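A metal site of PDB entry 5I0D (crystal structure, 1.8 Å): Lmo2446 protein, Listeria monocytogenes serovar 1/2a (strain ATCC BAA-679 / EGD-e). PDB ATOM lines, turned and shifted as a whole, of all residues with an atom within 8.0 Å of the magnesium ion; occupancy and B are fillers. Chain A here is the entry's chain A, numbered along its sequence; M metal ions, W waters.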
ATOM      1  N   ALA A 371      10.950  -6.465   3.123  1.00  0.00           N
ATOM      2  CA  ALA A 371      12.026  -5.775   2.388  1.00  0.00           C
ATOM      3  C   ALA A 371      12.410  -4.565   3.213  1.00  0.00           C
ATOM      4  O   ALA A 371      11.550  -3.763   3.556  1.00  0.00           O
ATOM      5  CB  ALA A 371      11.568  -5.324   1.004  1.00  0.00           C
ATOM      6  N   ASN A 372      13.696  -4.430   3.507  1.00  0.00           N
ATOM      7  CA  ASN A 372      14.148  -3.311   4.306  1.00  0.00           C
ATOM      8  C   ASN A 372      13.806  -1.959   3.654  1.00  0.00           C
ATOM      9  O   ASN A 372      13.559  -0.983   4.346  1.00  0.00           O
ATOM     10  CB  ASN A 372      15.636  -3.384   4.592  1.00  0.00           C
ATOM     11  CG  ASN A 372      16.068  -2.361   5.628  1.00  0.00           C
ATOM     12  OD1 ASN A 372      16.655  -1.308   5.301  1.00  0.00           O
ATOM     13  ND2 ASN A 372      15.720  -2.622   6.887  1.00  0.00           N
ATOM     14  N   GLU A 373      13.788  -1.917   2.330  1.00  0.00           N
ATOM     15  CA  GLU A 373      13.480  -0.692   1.601  1.00  0.00           C
ATOM     16  C   GLU A 373      12.066  -0.158   1.769  1.00  0.00           C
ATOM     17  O   GLU A 373      11.799   0.981   1.372  1.00  0.00           O
ATOM     18  CB  GLU A 373      13.819  -0.835   0.115  1.00  0.00           C
ATOM     19  CG  GLU A 373      12.954  -1.811  -0.656  1.00  0.00           C
ATOM     20  CD  GLU A 373      13.565  -2.174  -2.016  1.00  0.00           C
ATOM     21  OE1 GLU A 373      14.595  -2.881  -2.071  1.00  0.00           O
ATOM     22  OE2 GLU A 373      12.981  -1.764  -3.039  1.00  0.00           O
ATOM     23  N   TRP A 374      11.147  -0.987   2.298  1.00  0.00           N
ATOM     24  CA  TRP A 374       9.788  -0.529   2.537  1.00  0.00           C
ATOM     25  C   TRP A 374       9.788   0.380   3.742  1.00  0.00           C
ATOM     26  O   TRP A 374       9.955  -0.084   4.868  1.00  0.00           O
ATOM     27  CB  TRP A 374       8.817  -1.693   2.715  1.00  0.00           C
ATOM     28  CG  TRP A 374       8.689  -2.598   1.528  1.00  0.00           C
ATOM     29  CD1 TRP A 374       9.011  -2.321   0.212  1.00  0.00           C
ATOM     30  CD2 TRP A 374       8.177  -3.938   1.522  1.00  0.00           C
ATOM     31  NE1 TRP A 374       8.758  -3.414  -0.577  1.00  0.00           N
ATOM     32  CE2 TRP A 374       8.233  -4.412   0.201  1.00  0.00           C
ATOM     33  CE3 TRP A 374       7.667  -4.782   2.527  1.00  0.00           C
ATOM     34  CZ2 TRP A 374       7.826  -5.700  -0.158  1.00  0.00           C
ATOM     35  CZ3 TRP A 374       7.261  -6.061   2.171  1.00  0.00           C
ATOM     36  CH2 TRP A 374       7.353  -6.505   0.846  1.00  0.00           C
ATOM     37  N   ASP A 375       9.643   1.680   3.486  1.00  0.00           N
ATOM     38  CA  ASP A 375       9.835   2.679   4.512  1.00  0.00           C
ATOM     39  C   ASP A 375       8.811   3.806   4.519  1.00  0.00           C
ATOM     40  O   ASP A 375       9.052   4.849   5.120  1.00  0.00           O
ATOM     41  CB  ASP A 375      11.245   3.232   4.405  1.00  0.00           C
ATOM     42  CG  ASP A 375      11.448   4.123   3.196  1.00  0.00           C
ATOM     43  OD1 ASP A 375      10.867   3.877   2.097  1.00  0.00           O
ATOM     44  OD2 ASP A 375      12.209   5.096   3.336  1.00  0.00           O
ATOM     45  N   ARG A 376       7.678   3.596   3.863  1.00  0.00           N
ATOM     46  CA  ARG A 376       6.603   4.581   3.828  1.00  0.00           C
ATOM     47  C   ARG A 376       5.302   3.905   3.387  1.00  0.00           C
ATOM     48  O   ARG A 376       5.306   2.788   2.847  1.00  0.00           O
ATOM     49  CB  ARG A 376       6.961   5.748   2.897  1.00  0.00           C
ATOM     50  CG  ARG A 376       7.179   5.319   1.452  1.00  0.00           C
ATOM     51  CD  ARG A 376       7.994   6.353   0.701  1.00  0.00           C
ATOM     52  NE  ARG A 376       9.407   6.324   1.105  1.00  0.00           N
ATOM     53  CZ  ARG A 376      10.279   7.324   0.941  1.00  0.00           C
ATOM     54  NH1 ARG A 376       9.918   8.464   0.378  1.00  0.00           N
ATOM     55  NH2 ARG A 376      11.540   7.170   1.345  1.00  0.00           N
ATOM     56  N   SER A 378       3.319   4.470   0.924  1.00  0.00           N
ATOM     57  CA  SER A 378       3.207   4.153  -0.510  1.00  0.00           C
ATOM     58  C   SER A 378       3.952   2.862  -0.865  1.00  0.00           C
ATOM     59  O   SER A 378       3.533   2.149  -1.783  1.00  0.00           O
ATOM     60  CB  SER A 378       3.655   5.338  -1.379  1.00  0.00           C
ATOM     61  OG  SER A 378       5.022   5.615  -1.164  1.00  0.00           O
ATOM     62  N   ASP A 379       5.053   2.557  -0.150  1.00  0.00           N
ATOM     63  CA  ASP A 379       5.754   1.281  -0.363  1.00  0.00           C
ATOM     64  C   ASP A 379       4.874   0.111   0.076  1.00  0.00           C
ATOM     65  O   ASP A 379       4.821  -0.921  -0.608  1.00  0.00           O
ATOM     66  CB  ASP A 379       7.080   1.215   0.415  1.00  0.00           C
ATOM     67  CG  ASP A 379       8.196   2.080  -0.177  1.00  0.00           C
ATOM     68  OD1 ASP A 379       8.038   2.607  -1.305  1.00  0.00           O
ATOM     69  OD2 ASP A 379       9.266   2.228   0.488  1.00  0.00           O
ATOM     70  N   VAL A 380       4.196   0.251   1.207  1.00  0.00           N
ATOM     71  CA  VAL A 380       3.318  -0.809   1.697  1.00  0.00           C
ATOM     72  C   VAL A 380       2.191  -1.022   0.720  1.00  0.00           C
ATOM     73  O   VAL A 380       1.942  -2.142   0.321  1.00  0.00           O
ATOM     74  CB  VAL A 380       2.783  -0.540   3.118  1.00  0.00           C
ATOM     75  CG1 VAL A 380       1.786  -1.614   3.537  1.00  0.00           C
ATOM     76  CG2 VAL A 380       3.945  -0.454   4.093  1.00  0.00           C
ATOM     77  N   GLN A 401      11.933  -0.592   8.385  1.00  0.00           N
ATOM     78  CA  GLN A 401      12.272   0.810   8.283  1.00  0.00           C
ATOM     79  C   GLN A 401      11.013   1.663   8.504  1.00  0.00           C
ATOM     80  O   GLN A 401      10.562   2.417   7.631  1.00  0.00           O
ATOM     81  CB  GLN A 401      12.950   1.061   6.944  1.00  0.00           C
ATOM     82  CG  GLN A 401      13.721   2.377   6.899  1.00  0.00           C
ATOM     83  CD  GLN A 401      14.477   2.663   5.602  1.00  0.00           C
ATOM     84  OE1 GLN A 401      15.038   3.745   5.478  1.00  0.00           O
ATOM     85  NE2 GLN A 401      14.496   1.736   4.644  1.00  0.00           N
ATOM     86  N   LYS A 435       5.965  10.169   5.755  1.00  0.00           N
ATOM     87  CA  LYS A 435       5.996   8.777   5.332  1.00  0.00           C
ATOM     88  C   LYS A 435       4.880   7.912   5.923  1.00  0.00           C
ATOM     89  O   LYS A 435       4.537   6.894   5.332  1.00  0.00           O
ATOM     90  CB  LYS A 435       7.366   8.165   5.635  1.00  0.00           C
ATOM     91  CG  LYS A 435       8.489   8.777   4.796  1.00  0.00           C
ATOM     92  CD  LYS A 435       9.864   8.376   5.274  1.00  0.00           C
ATOM     93  CE  LYS A 435      10.927   8.995   4.387  1.00  0.00           C
ATOM     94  NZ  LYS A 435      12.272   8.885   5.020  1.00  0.00           N
ATOM     95  N   LYS A 664      18.932  -3.987   1.583  1.00  0.00           N
ATOM     96  CA  LYS A 664      19.210  -2.574   1.273  1.00  0.00           C
ATOM     97  C   LYS A 664      18.060  -1.625   1.605  1.00  0.00           C
ATOM     98  O   LYS A 664      16.908  -1.976   1.453  1.00  0.00           O
ATOM     99  CB  LYS A 664      19.713  -2.401  -0.158  1.00  0.00           C
ATOM    100  CG  LYS A 664      21.110  -2.968  -0.275  1.00  0.00           C
ATOM    101  CD  LYS A 664      21.795  -2.504  -1.524  1.00  0.00           C
ATOM    102  CE  LYS A 664      23.239  -2.981  -1.530  1.00  0.00           C
ATOM    103  NZ  LYS A 664      23.872  -2.522  -2.784  1.00  0.00           N
ATOM    104  N   SER A 665      18.393  -0.448   2.117  1.00  0.00           N
ATOM    105  CA  SER A 665      17.388   0.457   2.682  1.00  0.00           C
ATOM    106  C   SER A 665      16.764   1.393   1.647  1.00  0.00           C
ATOM    107  O   SER A 665      15.622   1.821   1.833  1.00  0.00           O
ATOM    108  CB  SER A 665      17.977   1.266   3.846  1.00  0.00           C
ATOM    109  OG  SER A 665      18.938   2.174   3.361  1.00  0.00           O
ATOM    110  N   ASP A 666      17.490   1.731   0.580  1.00  0.00           N
ATOM    111  CA  ASP A 666      16.920   2.612  -0.454  1.00  0.00           C
ATOM    112  C   ASP A 666      17.606   2.420  -1.811  1.00  0.00           C
ATOM    113  O   ASP A 666      18.174   3.355  -2.379  1.00  0.00           O
ATOM    114  CB  ASP A 666      17.000   4.076   0.020  1.00  0.00           C
ATOM    115  CG  ASP A 666      16.308   5.064  -0.924  1.00  0.00           C
ATOM    116  OD1 ASP A 666      15.340   4.699  -1.617  1.00  0.00           O
ATOM    117  OD2 ASP A 666      16.735   6.242  -0.953  1.00  0.00           O
ATOM    118  N   PRO A 667      17.554   1.201  -2.351  1.00  0.00           N
ATOM    119  CA  PRO A 667      18.311   0.880  -3.562  1.00  0.00           C
ATOM    120  C   PRO A 667      17.569   1.242  -4.857  1.00  0.00           C
ATOM    121  O   PRO A 667      16.357   1.324  -4.869  1.00  0.00           O
ATOM    122  CB  PRO A 667      18.448  -0.623  -3.469  1.00  0.00           C
ATOM    123  CG  PRO A 667      17.160  -1.044  -2.863  1.00  0.00           C
ATOM    124  CD  PRO A 667      16.781   0.026  -1.884  1.00  0.00           C
HETATM  125 MG    MG M   1      11.378   2.813   0.256  1.00  0.00          MG
HETATM  126  O   HOH W   1      13.445   3.314   0.697  1.00  0.00           O
HETATM  127  O   HOH W   2      11.252   1.614  -1.480  1.00  0.00           O
HETATM  128  O   HOH W   3      10.728   4.383  -0.877  1.00  0.00           O
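The magnesium ion is bound by water W3, water W2, water W1, O of Glu 373, OD1 of Asp 375 and OD2 of Asp 379.
The magnesium ion has six donor atoms within binding distance.
The backbone NH (N) of Glu 373 is in hydrogen-bond range of the backbone carbonyl oxygen (O) of Lys 664 (3.2 Å).
NH2 of Arg 376 is in salt-bridge range of OD2 of Asp 375.
Water W3 bridges NE of Arg 376 and OD1 of Asp 379.
The nearest printed residue that does not touch the magnesium ion is Arg 376 (4.1 Å).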
